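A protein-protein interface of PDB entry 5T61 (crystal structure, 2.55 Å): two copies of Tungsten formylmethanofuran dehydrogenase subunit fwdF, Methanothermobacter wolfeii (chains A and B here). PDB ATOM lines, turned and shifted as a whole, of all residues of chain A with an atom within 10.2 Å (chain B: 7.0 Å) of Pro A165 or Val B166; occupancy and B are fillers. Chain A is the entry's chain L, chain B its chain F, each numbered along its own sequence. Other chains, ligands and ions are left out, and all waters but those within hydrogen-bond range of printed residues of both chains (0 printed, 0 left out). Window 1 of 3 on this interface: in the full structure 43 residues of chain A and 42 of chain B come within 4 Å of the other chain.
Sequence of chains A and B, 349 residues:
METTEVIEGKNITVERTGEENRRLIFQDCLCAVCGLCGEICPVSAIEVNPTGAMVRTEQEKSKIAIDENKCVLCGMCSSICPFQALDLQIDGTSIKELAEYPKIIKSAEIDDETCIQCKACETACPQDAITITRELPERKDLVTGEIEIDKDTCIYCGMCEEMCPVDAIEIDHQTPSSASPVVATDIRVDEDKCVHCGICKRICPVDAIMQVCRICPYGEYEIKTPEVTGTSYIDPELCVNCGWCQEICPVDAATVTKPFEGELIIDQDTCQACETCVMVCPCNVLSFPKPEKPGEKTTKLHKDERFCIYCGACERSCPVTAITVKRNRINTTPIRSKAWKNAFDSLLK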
ATOM      1  N   ARG A 139     -28.786  31.952  19.169  1.00  0.00           N
ATOM      2  CA  ARG A 139     -28.277  31.099  18.101  1.00  0.00           C
ATOM      3  C   ARG A 139     -28.212  29.643  18.544  1.00  0.00           C
ATOM      4  O   ARG A 139     -28.612  28.734  17.805  1.00  0.00           O
ATOM      5  CB  ARG A 139     -26.901  31.604  17.676  1.00  0.00           C
ATOM      6  CG  ARG A 139     -26.248  30.860  16.537  1.00  0.00           C
ATOM      7  CD  ARG A 139     -25.391  31.824  15.744  1.00  0.00           C
ATOM      8  NE  ARG A 139     -24.010  31.822  16.211  1.00  0.00           N
ATOM      9  CZ  ARG A 139     -23.159  32.824  16.018  1.00  0.00           C
ATOM     10  NH1 ARG A 139     -21.917  32.740  16.478  1.00  0.00           N
ATOM     11  NH2 ARG A 139     -23.549  33.913  15.369  1.00  0.00           N
ATOM     12  N   ILE A 147     -19.881  18.533  20.190  1.00  0.00           N
ATOM     13  CA  ILE A 147     -18.522  18.828  19.747  1.00  0.00           C
ATOM     14  C   ILE A 147     -17.590  18.844  20.952  1.00  0.00           C
ATOM     15  O   ILE A 147     -17.886  19.464  21.978  1.00  0.00           O
ATOM     16  CB  ILE A 147     -18.451  20.152  18.955  1.00  0.00           C
ATOM     17  CG1 ILE A 147     -17.034  20.380  18.422  1.00  0.00           C
ATOM     18  CG2 ILE A 147     -18.948  21.332  19.792  1.00  0.00           C
ATOM     19  CD1 ILE A 147     -16.969  21.407  17.315  1.00  0.00           C
ATOM     20  N   MET A 159      -5.377  25.356  12.497  1.00  0.00           N
ATOM     21  CA  MET A 159      -6.163  25.301  11.264  1.00  0.00           C
ATOM     22  C   MET A 159      -7.666  25.360  11.539  1.00  0.00           C
ATOM     23  O   MET A 159      -8.412  25.978  10.771  1.00  0.00           O
ATOM     24  CB  MET A 159      -5.809  24.052  10.452  1.00  0.00           C
ATOM     25  CG  MET A 159      -4.441  24.112   9.760  1.00  0.00           C
ATOM     26  SD  MET A 159      -4.151  22.784   8.555  1.00  0.00           S
ATOM     27  CE  MET A 159      -3.193  21.577   9.458  1.00  0.00           C
ATOM     28  N   CYS A 160      -8.132  24.746  12.628  1.00  0.00           N
ATOM     29  CA  CYS A 160      -9.559  24.813  12.932  1.00  0.00           C
ATOM     30  C   CYS A 160      -9.965  26.212  13.367  1.00  0.00           C
ATOM     31  O   CYS A 160     -11.026  26.708  12.974  1.00  0.00           O
ATOM     32  CB  CYS A 160      -9.919  23.835  14.041  1.00  0.00           C
ATOM     33  SG  CYS A 160      -9.531  24.544  15.651  1.00  0.00           S
ATOM     34  N   GLU A 161      -9.131  26.857  14.187  1.00  0.00           N
ATOM     35  CA  GLU A 161      -9.415  28.219  14.623  1.00  0.00           C
ATOM     36  C   GLU A 161      -9.528  29.159  13.432  1.00  0.00           C
ATOM     37  O   GLU A 161     -10.399  30.035  13.402  1.00  0.00           O
ATOM     38  CB  GLU A 161      -8.329  28.689  15.590  1.00  0.00           C
ATOM     39  CG  GLU A 161      -8.557  30.068  16.178  1.00  0.00           C
ATOM     40  CD  GLU A 161      -7.374  30.557  16.991  1.00  0.00           C
ATOM     41  OE1 GLU A 161      -7.601  31.191  18.044  1.00  0.00           O
ATOM     42  OE2 GLU A 161      -6.221  30.308  16.579  1.00  0.00           O
ATOM     43  N   GLU A 162      -8.652  28.988  12.442  1.00  0.00           N
ATOM     44  CA  GLU A 162      -8.707  29.812  11.241  1.00  0.00           C
ATOM     45  C   GLU A 162      -9.968  29.526  10.432  1.00  0.00           C
ATOM     46  O   GLU A 162     -10.663  30.454  10.002  1.00  0.00           O
ATOM     47  CB  GLU A 162      -7.456  29.579  10.398  1.00  0.00           C
ATOM     48  CG  GLU A 162      -6.257  30.391  10.859  1.00  0.00           C
ATOM     49  CD  GLU A 162      -4.998  30.064  10.088  1.00  0.00           C
ATOM     50  OE1 GLU A 162      -5.072  29.954   8.847  1.00  0.00           O
ATOM     51  OE2 GLU A 162      -3.931  29.924  10.725  1.00  0.00           O
ATOM     52  N   MET A 163     -10.278  28.247  10.213  1.00  0.00           N
ATOM     53  CA  MET A 163     -11.378  27.872   9.331  1.00  0.00           C
ATOM     54  C   MET A 163     -12.757  28.057   9.955  1.00  0.00           C
ATOM     55  O   MET A 163     -13.735  28.180   9.209  1.00  0.00           O
ATOM     56  CB  MET A 163     -11.233  26.419   8.875  1.00  0.00           C
ATOM     57  CG  MET A 163      -9.970  26.144   8.099  1.00  0.00           C
ATOM     58  SD  MET A 163     -10.136  26.759   6.421  1.00  0.00           S
ATOM     59  CE  MET A 163     -11.285  25.582   5.738  1.00  0.00           C
ATOM     60  N   CYS A 164     -12.868  28.059  11.288  1.00  0.00           N
ATOM     61  CA  CYS A 164     -14.171  28.168  11.934  1.00  0.00           C
ATOM     62  C   CYS A 164     -14.893  29.424  11.465  1.00  0.00           C
ATOM     63  O   CYS A 164     -14.440  30.541  11.740  1.00  0.00           O
ATOM     64  CB  CYS A 164     -14.034  28.194  13.455  1.00  0.00           C
ATOM     65  SG  CYS A 164     -15.476  28.914  14.275  1.00  0.00           S
ATOM     66  N   PRO A 165     -16.019  29.284  10.757  1.00  0.00           N
ATOM     67  CA  PRO A 165     -16.646  30.461  10.139  1.00  0.00           C
ATOM     68  C   PRO A 165     -17.364  31.365  11.124  1.00  0.00           C
ATOM     69  O   PRO A 165     -17.763  32.471  10.734  1.00  0.00           O
ATOM     70  CB  PRO A 165     -17.624  29.841   9.136  1.00  0.00           C
ATOM     71  CG  PRO A 165     -18.003  28.532   9.758  1.00  0.00           C
ATOM     72  CD  PRO A 165     -16.790  28.049  10.517  1.00  0.00           C
ATOM     73  N   VAL A 166     -17.546  30.941  12.375  1.00  0.00           N
ATOM     74  CA  VAL A 166     -18.179  31.767  13.392  1.00  0.00           C
ATOM     75  C   VAL A 166     -17.235  32.082  14.549  1.00  0.00           C
ATOM     76  O   VAL A 166     -17.686  32.555  15.594  1.00  0.00           O
ATOM     77  CB  VAL A 166     -19.483  31.125  13.910  1.00  0.00           C
ATOM     78  CG1 VAL A 166     -20.420  30.809  12.750  1.00  0.00           C
ATOM     79  CG2 VAL A 166     -19.197  29.880  14.744  1.00  0.00           C
ATOM     80  N   ASP A 167     -15.931  31.832  14.384  1.00  0.00           N
ATOM     81  CA  ASP A 167     -14.933  32.069  15.434  1.00  0.00           C
ATOM     82  C   ASP A 167     -15.357  31.447  16.766  1.00  0.00           C
ATOM     83  O   ASP A 167     -15.245  32.060  17.830  1.00  0.00           O
ATOM     84  CB  ASP A 167     -14.689  33.570  15.601  1.00  0.00           C
ATOM     85  CG  ASP A 167     -14.271  34.242  14.315  1.00  0.00           C
ATOM     86  OD1 ASP A 167     -13.473  33.648  13.562  1.00  0.00           O
ATOM     87  OD2 ASP A 167     -14.791  35.342  14.031  1.00  0.00           O
ATOM     88  N   ALA A 168     -15.842  30.203  16.705  1.00  0.00           N
ATOM     89  CA  ALA A 168     -16.245  29.499  17.918  1.00  0.00           C
ATOM     90  C   ALA A 168     -15.080  28.843  18.649  1.00  0.00           C
ATOM     91  O   ALA A 168     -15.186  28.579  19.852  1.00  0.00           O
ATOM     92  CB  ALA A 168     -17.299  28.439  17.589  1.00  0.00           C
ATOM     93  N   ILE A 169     -13.981  28.579  17.964  1.00  0.00           N
ATOM     94  CA  ILE A 169     -12.836  27.914  18.566  1.00  0.00           C
ATOM     95  C   ILE A 169     -11.838  28.967  19.019  1.00  0.00           C
ATOM     96  O   ILE A 169     -11.576  29.946  18.306  1.00  0.00           O
ATOM     97  CB  ILE A 169     -12.198  26.919  17.580  1.00  0.00           C
ATOM     98  CG1 ILE A 169     -13.185  25.786  17.293  1.00  0.00           C
ATOM     99  CG2 ILE A 169     -10.900  26.382  18.149  1.00  0.00           C
ATOM    100  CD1 ILE A 169     -12.837  24.940  16.099  1.00  0.00           C
ATOM    101  N   VAL A 189     -14.045  25.203  22.488  1.00  0.00           N
ATOM    102  CA  VAL A 189     -15.139  25.488  21.567  1.00  0.00           C
ATOM    103  C   VAL A 189     -16.235  26.213  22.334  1.00  0.00           C
ATOM    104  O   VAL A 189     -16.684  25.735  23.383  1.00  0.00           O
ATOM    105  CB  VAL A 189     -15.697  24.204  20.930  1.00  0.00           C
ATOM    106  CG1 VAL A 189     -16.879  24.531  20.022  1.00  0.00           C
ATOM    107  CG2 VAL A 189     -14.617  23.482  20.168  1.00  0.00           C
ATOM    108  N   LYS A 193     -21.695  29.756  20.144  1.00  0.00           N
ATOM    109  CA  LYS A 193     -21.445  30.241  18.794  1.00  0.00           C
ATOM    110  C   LYS A 193     -21.450  29.140  17.748  1.00  0.00           C
ATOM    111  O   LYS A 193     -21.881  29.382  16.619  1.00  0.00           O
ATOM    112  CB  LYS A 193     -20.103  30.975  18.745  1.00  0.00           C
ATOM    113  CG  LYS A 193     -20.062  32.179  19.666  1.00  0.00           C
ATOM    114  CD  LYS A 193     -18.899  33.092  19.353  1.00  0.00           C
ATOM    115  CE  LYS A 193     -18.747  34.146  20.433  1.00  0.00           C
ATOM    116  NZ  LYS A 193     -17.558  35.004  20.199  1.00  0.00           N
ATOM    117  N   CYS A 194     -20.985  27.944  18.107  1.00  0.00           N
ATOM    118  CA  CYS A 194     -20.901  26.826  17.177  1.00  0.00           C
ATOM    119  C   CYS A 194     -22.251  26.533  16.532  1.00  0.00           C
ATOM    120  O   CYS A 194     -23.271  26.417  17.219  1.00  0.00           O
ATOM    121  CB  CYS A 194     -20.384  25.595  17.932  1.00  0.00           C
ATOM    122  SG  CYS A 194     -20.803  23.975  17.247  1.00  0.00           S
ATOM    123  N   VAL A 195     -22.251  26.414  15.203  1.00  0.00           N
ATOM    124  CA  VAL A 195     -23.437  26.040  14.441  1.00  0.00           C
ATOM    125  C   VAL A 195     -23.285  24.667  13.798  1.00  0.00           C
ATOM    126  O   VAL A 195     -24.083  24.305  12.925  1.00  0.00           O
ATOM    127  CB  VAL A 195     -23.788  27.105  13.384  1.00  0.00           C
ATOM    128  CG1 VAL A 195     -23.927  28.474  14.033  1.00  0.00           C
ATOM    129  CG2 VAL A 195     -22.736  27.138  12.282  1.00  0.00           C
ATOM    130  N   HIS A 196     -22.268  23.897  14.202  1.00  0.00           N
ATOM    131  CA  HIS A 196     -22.113  22.490  13.821  1.00  0.00           C
ATOM    132  C   HIS A 196     -22.055  22.299  12.305  1.00  0.00           C
ATOM    133  O   HIS A 196     -22.756  21.457  11.738  1.00  0.00           O
ATOM    134  CB  HIS A 196     -23.235  21.650  14.440  1.00  0.00           C
ATOM    135  CG  HIS A 196     -23.187  21.606  15.936  1.00  0.00           C
ATOM    136  ND1 HIS A 196     -22.223  20.899  16.624  1.00  0.00           N
ATOM    137  CD2 HIS A 196     -23.948  22.217  16.876  1.00  0.00           C
ATOM    138  CE1 HIS A 196     -22.407  21.058  17.922  1.00  0.00           C
ATOM    139  NE2 HIS A 196     -23.447  21.851  18.103  1.00  0.00           N
ATOM    140  N   CYS A 197     -21.195  23.079  11.644  1.00  0.00           N
ATOM    141  CA  CYS A 197     -21.044  22.928  10.203  1.00  0.00           C
ATOM    142  C   CYS A 197     -20.084  21.805   9.822  1.00  0.00           C
ATOM    143  O   CYS A 197     -20.137  21.333   8.682  1.00  0.00           O
ATOM    144  CB  CYS A 197     -20.590  24.235   9.550  1.00  0.00           C
ATOM    145  SG  CYS A 197     -18.852  24.623   9.702  1.00  0.00           S
ATOM    146  N   GLY A 198     -19.195  21.390  10.725  1.00  0.00           N
ATOM    147  CA  GLY A 198     -18.316  20.266  10.473  1.00  0.00           C
ATOM    148  C   GLY A 198     -16.959  20.609   9.898  1.00  0.00           C
ATOM    149  O   GLY A 198     -16.152  19.696   9.677  1.00  0.00           O
ATOM    150  N   ILE A 199     -16.686  21.889   9.635  1.00  0.00           N
ATOM    151  CA  ILE A 199     -15.452  22.266   8.948  1.00  0.00           C
ATOM    152  C   ILE A 199     -14.231  21.897   9.785  1.00  0.00           C
ATOM    153  O   ILE A 199     -13.257  21.329   9.270  1.00  0.00           O
ATOM    154  CB  ILE A 199     -15.477  23.764   8.587  1.00  0.00           C
ATOM    155  CG1 ILE A 199     -16.355  23.996   7.353  1.00  0.00           C
ATOM    156  CG2 ILE A 199     -14.079  24.290   8.353  1.00  0.00           C
ATOM    157  CD1 ILE A 199     -16.675  25.449   7.082  1.00  0.00           C
ATOM    158  N   CYS A 200     -14.259  22.222  11.083  1.00  0.00           N
ATOM    159  CA  CYS A 200     -13.094  22.003  11.940  1.00  0.00           C
ATOM    160  C   CYS A 200     -12.665  20.543  11.927  1.00  0.00           C
ATOM    161  O   CYS A 200     -11.475  20.233  11.810  1.00  0.00           O
ATOM    162  CB  CYS A 200     -13.399  22.418  13.376  1.00  0.00           C
ATOM    163  SG  CYS A 200     -14.540  21.278  14.188  1.00  0.00           S
ATOM    164  N   LYS A 201     -13.626  19.630  12.090  1.00  0.00           N
ATOM    165  CA  LYS A 201     -13.303  18.211  12.146  1.00  0.00           C
ATOM    166  C   LYS A 201     -12.730  17.706  10.825  1.00  0.00           C
ATOM    167  O   LYS A 201     -11.840  16.850  10.827  1.00  0.00           O
ATOM    168  CB  LYS A 201     -14.546  17.421  12.569  1.00  0.00           C
ATOM    169  CG  LYS A 201     -14.838  16.163  11.770  1.00  0.00           C
ATOM    170  CD  LYS A 201     -16.128  15.509  12.247  1.00  0.00           C
ATOM    171  CE  LYS A 201     -17.304  15.913  11.366  1.00  0.00           C
ATOM    172  NZ  LYS A 201     -18.520  15.086  11.612  1.00  0.00           N
ATOM    173  N   ARG A 202     -13.192  18.242   9.690  1.00  0.00           N
ATOM    174  CA  ARG A 202     -12.640  17.812   8.405  1.00  0.00           C
ATOM    175  C   ARG A 202     -11.234  18.349   8.174  1.00  0.00           C
ATOM    176  O   ARG A 202     -10.425  17.690   7.512  1.00  0.00           O
ATOM    177  CB  ARG A 202     -13.560  18.220   7.252  1.00  0.00           C
ATOM    178  CG  ARG A 202     -14.803  17.357   7.117  1.00  0.00           C
ATOM    179  CD  ARG A 202     -15.670  17.767   5.934  1.00  0.00           C
ATOM    180  NE  ARG A 202     -16.511  18.916   6.243  1.00  0.00           N
ATOM    181  CZ  ARG A 202     -17.726  18.804   6.772  1.00  0.00           C
ATOM    182  NH1 ARG A 202     -18.450  19.885   7.035  1.00  0.00           N
ATOM    183  NH2 ARG A 202     -18.214  17.598   7.036  1.00  0.00           N
ATOM    184  N   ILE A 203     -10.914  19.527   8.708  1.00  0.00           N
ATOM    185  CA  ILE A 203      -9.596  20.105   8.475  1.00  0.00           C
ATOM    186  C   ILE A 203      -8.554  19.604   9.471  1.00  0.00           C
ATOM    187  O   ILE A 203      -7.350  19.697   9.191  1.00  0.00           O
ATOM    188  CB  ILE A 203      -9.663  21.644   8.508  1.00  0.00           C
ATOM    189  CG1 ILE A 203      -8.414  22.253   7.872  1.00  0.00           C
ATOM    190  CG2 ILE A 203      -9.796  22.146   9.937  1.00  0.00           C
ATOM    191  CD1 ILE A 203      -8.266  21.907   6.416  1.00  0.00           C
ATOM    192  N   ARG B 139     -13.642  27.531   1.926  1.00  0.00           N
ATOM    193  CA  ARG B 139     -14.760  27.130   2.772  1.00  0.00           C
ATOM    194  C   ARG B 139     -15.846  26.433   1.959  1.00  0.00           C
ATOM    195  O   ARG B 139     -16.377  25.394   2.371  1.00  0.00           O
ATOM    196  CB  ARG B 139     -15.305  28.362   3.492  1.00  0.00           C
ATOM    197  CG  ARG B 139     -16.412  28.106   4.487  1.00  0.00           C
ATOM    198  CD  ARG B 139     -16.298  29.107   5.629  1.00  0.00           C
ATOM    199  NE  ARG B 139     -17.126  30.290   5.413  1.00  0.00           N
ATOM    200  CZ  ARG B 139     -16.917  31.467   5.994  1.00  0.00           C
ATOM    201  NH1 ARG B 139     -17.725  32.483   5.736  1.00  0.00           N
ATOM    202  NH2 ARG B 139     -15.899  31.629   6.826  1.00  0.00           N
ATOM    203  N   MET B 163     -29.401  37.219  11.885  1.00  0.00           N
ATOM    204  CA  MET B 163     -29.076  35.950  12.529  1.00  0.00           C
ATOM    205  C   MET B 163     -27.962  35.185  11.828  1.00  0.00           C
ATOM    206  O   MET B 163     -27.316  34.347  12.468  1.00  0.00           O
ATOM    207  CB  MET B 163     -30.310  35.047  12.604  1.00  0.00           C
ATOM    208  CG  MET B 163     -31.483  35.629  13.362  1.00  0.00           C
ATOM    209  SD  MET B 163     -31.284  35.551  15.145  1.00  0.00           S
ATOM    210  CE  MET B 163     -31.493  33.810  15.441  1.00  0.00           C
ATOM    211  N   CYS B 164     -27.732  35.434  10.536  1.00  0.00           N
ATOM    212  CA  CYS B 164     -26.740  34.677   9.783  1.00  0.00           C
ATOM    213  C   CYS B 164     -25.371  34.776  10.445  1.00  0.00           C
ATOM    214  O   CYS B 164     -24.769  35.855  10.479  1.00  0.00           O
ATOM    215  CB  CYS B 164     -26.671  35.173   8.338  1.00  0.00           C
ATOM    216  SG  CYS B 164     -25.146  34.717   7.507  1.00  0.00           S
ATOM    217  N   PRO B 165     -24.841  33.666  10.967  1.00  0.00           N
ATOM    218  CA  PRO B 165     -23.620  33.740  11.781  1.00  0.00           C
ATOM    219  C   PRO B 165     -22.346  33.959  10.983  1.00  0.00           C
ATOM    220  O   PRO B 165     -21.303  34.242  11.587  1.00  0.00           O
ATOM    221  CB  PRO B 165     -23.599  32.380  12.488  1.00  0.00           C
ATOM    222  CG  PRO B 165     -24.284  31.461  11.531  1.00  0.00           C
ATOM    223  CD  PRO B 165     -25.325  32.281  10.811  1.00  0.00           C
ATOM    224  N   VAL B 166     -22.397  33.845   9.657  1.00  0.00           N
ATOM    225  CA  VAL B 166     -21.248  34.100   8.804  1.00  0.00           C
ATOM    226  C   VAL B 166     -21.485  35.285   7.877  1.00  0.00           C
ATOM    227  O   VAL B 166     -20.672  35.547   6.991  1.00  0.00           O
ATOM    228  CB  VAL B 166     -20.858  32.839   8.006  1.00  0.00           C
ATOM    229  CG1 VAL B 166     -20.654  31.661   8.956  1.00  0.00           C
ATOM    230  CG2 VAL B 166     -21.908  32.524   6.961  1.00  0.00           C
ATOM    231  N   ASP B 167     -22.555  36.041   8.106  1.00  0.00           N
ATOM    232  CA  ASP B 167     -22.912  37.203   7.289  1.00  0.00           C
ATOM    233  C   ASP B 167     -22.891  36.880   5.797  1.00  0.00           C
ATOM    234  O   ASP B 167     -22.367  37.633   4.973  1.00  0.00           O
ATOM    235  CB  ASP B 167     -22.016  38.388   7.638  1.00  0.00           C
ATOM    236  CG  ASP B 167     -22.071  38.726   9.121  1.00  0.00           C
ATOM    237  OD1 ASP B 167     -21.516  39.755   9.546  1.00  0.00           O
ATOM    238  OD2 ASP B 167     -22.666  37.936   9.881  1.00  0.00           O
ATOM    239  N   ALA B 168     -23.509  35.752   5.442  1.00  0.00           N
ATOM    240  CA  ALA B 168     -23.624  35.382   4.033  1.00  0.00           C
ATOM    241  C   ALA B 168     -24.771  36.096   3.328  1.00  0.00           C
ATOM    242  O   ALA B 168     -24.753  36.202   2.098  1.00  0.00           O
ATOM    243  CB  ALA B 168     -23.800  33.868   3.898  1.00  0.00           C
ATOM    244  N   ILE B 169     -25.756  36.589   4.072  1.00  0.00           N
ATOM    245  CA  ILE B 169     -26.925  37.244   3.496  1.00  0.00           C
ATOM    246  C   ILE B 169     -26.719  38.752   3.506  1.00  0.00           C
ATOM    247  O   ILE B 169     -26.205  39.321   4.478  1.00  0.00           O
ATOM    248  CB  ILE B 169     -28.203  36.844   4.254  1.00  0.00           C
ATOM    249  CG1 ILE B 169     -28.465  35.347   4.056  1.00  0.00           C
ATOM    250  CG2 ILE B 169     -29.381  37.656   3.758  1.00  0.00           C
ATOM    251  CD1 ILE B 169     -29.486  34.757   4.997  1.00  0.00           C
ATOM    252  N   ASP B 190     -24.546  34.812  -0.316  1.00  0.00           N
ATOM    253  CA  ASP B 190     -23.209  34.527  -0.831  1.00  0.00           C
ATOM    254  C   ASP B 190     -22.880  33.078  -0.485  1.00  0.00           C
ATOM    255  O   ASP B 190     -22.493  32.772   0.645  1.00  0.00           O
ATOM    256  CB  ASP B 190     -22.201  35.508  -0.243  1.00  0.00           C
ATOM    257  CG  ASP B 190     -20.810  35.349  -0.825  1.00  0.00           C
ATOM    258  OD1 ASP B 190     -20.577  34.409  -1.615  1.00  0.00           O
ATOM    259  OD2 ASP B 190     -19.943  36.183  -0.496  1.00  0.00           O
ATOM    260  N   LYS B 193     -19.793  31.819   1.261  1.00  0.00           N
ATOM    261  CA  LYS B 193     -19.719  31.994   2.709  1.00  0.00           C
ATOM    262  C   LYS B 193     -20.683  31.096   3.478  1.00  0.00           C
ATOM    263  O   LYS B 193     -20.365  30.671   4.596  1.00  0.00           O
ATOM    264  CB  LYS B 193     -19.989  33.457   3.081  1.00  0.00           C
ATOM    265  CG  LYS B 193     -18.971  34.441   2.518  1.00  0.00           C
ATOM    266  CD  LYS B 193     -19.062  35.794   3.219  1.00  0.00           C
ATOM    267  CE  LYS B 193     -18.213  36.836   2.505  1.00  0.00           C
ATOM    268  NZ  LYS B 193     -18.342  38.189   3.115  1.00  0.00           N
ATOM    269  N   CYS B 194     -21.855  30.818   2.912  1.00  0.00           N
ATOM    270  CA  CYS B 194     -22.861  29.987   3.564  1.00  0.00           C
ATOM    271  C   CYS B 194     -22.313  28.609   3.943  1.00  0.00           C
ATOM    272  O   CYS B 194     -21.689  27.931   3.122  1.00  0.00           O
ATOM    273  CB  CYS B 194     -24.058  29.852   2.620  1.00  0.00           C
ATOM    274  SG  CYS B 194     -25.072  28.394   2.864  1.00  0.00           S
ATOM    275  N   VAL B 195     -22.552  28.195   5.189  1.00  0.00           N
ATOM    276  CA  VAL B 195     -22.199  26.851   5.654  1.00  0.00           C
ATOM    277  C   VAL B 195     -23.437  26.015   5.953  1.00  0.00           C
ATOM    278  O   VAL B 195     -23.328  24.952   6.576  1.00  0.00           O
ATOM    279  CB  VAL B 195     -21.266  26.890   6.877  1.00  0.00           C
ATOM    280  CG1 VAL B 195     -20.038  27.742   6.584  1.00  0.00           C
ATOM    281  CG2 VAL B 195     -22.002  27.388   8.114  1.00  0.00           C
ATOM    282  N   HIS B 196     -24.618  26.479   5.534  1.00  0.00           N
ATOM    283  CA  HIS B 196     -25.850  25.690   5.553  1.00  0.00           C
ATOM    284  C   HIS B 196     -26.218  25.208   6.956  1.00  0.00           C
ATOM    285  O   HIS B 196     -26.492  24.028   7.181  1.00  0.00           O
ATOM    286  CB  HIS B 196     -25.722  24.512   4.587  1.00  0.00           C
ATOM    287  CG  HIS B 196     -25.510  24.928   3.166  1.00  0.00           C
ATOM    288  ND1 HIS B 196     -26.498  25.511   2.402  1.00  0.00           N
ATOM    289  CD2 HIS B 196     -24.408  24.879   2.380  1.00  0.00           C
ATOM    290  CE1 HIS B 196     -26.022  25.780   1.198  1.00  0.00           C
ATOM    291  NE2 HIS B 196     -24.754  25.410   1.162  1.00  0.00           N
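The guanidinium group (NE) of Arg B139 lies within hydrogen-bond range of the backbone carbonyl oxygen (O) of Lys B193.
The backbone NH of Val B166 sits close to the side-chain sulfur of Cys B164 (3.6 Å).
NE of Arg A139 lies within hydrogen-bond range of O of Lys A193, at 3.3 Å.
SG of Cys A164 sits close to N of Val A166, 3.5 Å away.
The side-chain sulfur of Cys A197 sits close to the backbone NH of Ile A199, at 3.5 Å.
O of Cys A197 sits at hydrogen-bond distance from NH1 of Arg A202, 2.8 Å away.
Pro B165 touches Arg A139.
Arg B139 touches Pro A165 (NH2 to CB, 3.4 Å).
CG1 of Val B166 touches O of Pro A165 (3.5 Å).
CG of Pro A165 touches CG1 of Val B195, 3.9 Å away.
Val A166 touches Pro B165 (CG1 to CB, 3.6 Å).
Val A166 touches Val B166.
CG1 of Val A195 touches CG of Pro B165, 3.9 Å away.
Val B195 touches Cys A197.
Arg B139 touches Ile A199.
Of chain A, only Pro A165 and Val A166 come within 4 Å of Val B166.
Of chain A, only Arg A139 (3.3 Å), Val A166 (3.6 Å) and Val A195 (3.9 Å) come within 4 Å of Pro B165.
No residue of chain A comes within 4 Å of Lys B193.
Of the printed residues of chain A, Arg B139 touches Pro A165 and Ile A199.
Printed residues of chain B within 4 Å of Val A166: Pro B165 (3.6 Å) and Val B166 (3.9 Å).
Printed residues of chain B within 4 Å of Cys A197: Val B195.
Printed residues of chain B within 4 Å of Arg A139: Pro B165 (3.3 Å).
The nearest residue of chain A that does not touch Val B166 is Arg A139 (5.8 Å).
Hydrophobic or aromatic side chains of chain A that line the printed part of chain B: Pro A165, Val A166, Val A195 and Ile A199.
Printed residues of chain B that touch a printed residue of chain A: Arg B139, Pro B165, Val B166 and Val B195.
Hydrophobic or aromatic side chains of chain B that line the printed part of chain A: Pro B165, Val B166 and Val B195.
Along chain B the printed residues that touch a printed residue of chain A span positions 139 to 195.
Arg A139 touches Pro B165, and with the chains exchanged Pro A165 touches Arg B139.
Pro A165 touches Val B166, and with the chains exchanged Val A166 touches Pro B165.
Pro A165 touches Val B195, and with the chains exchanged Val A195 touches Pro B165.
Val A166 touches its own counterpart, Val B166.
Of the 9 pairs that touch across the chains among the printed residues, 7 have their exchanged pair printed and touching as well.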
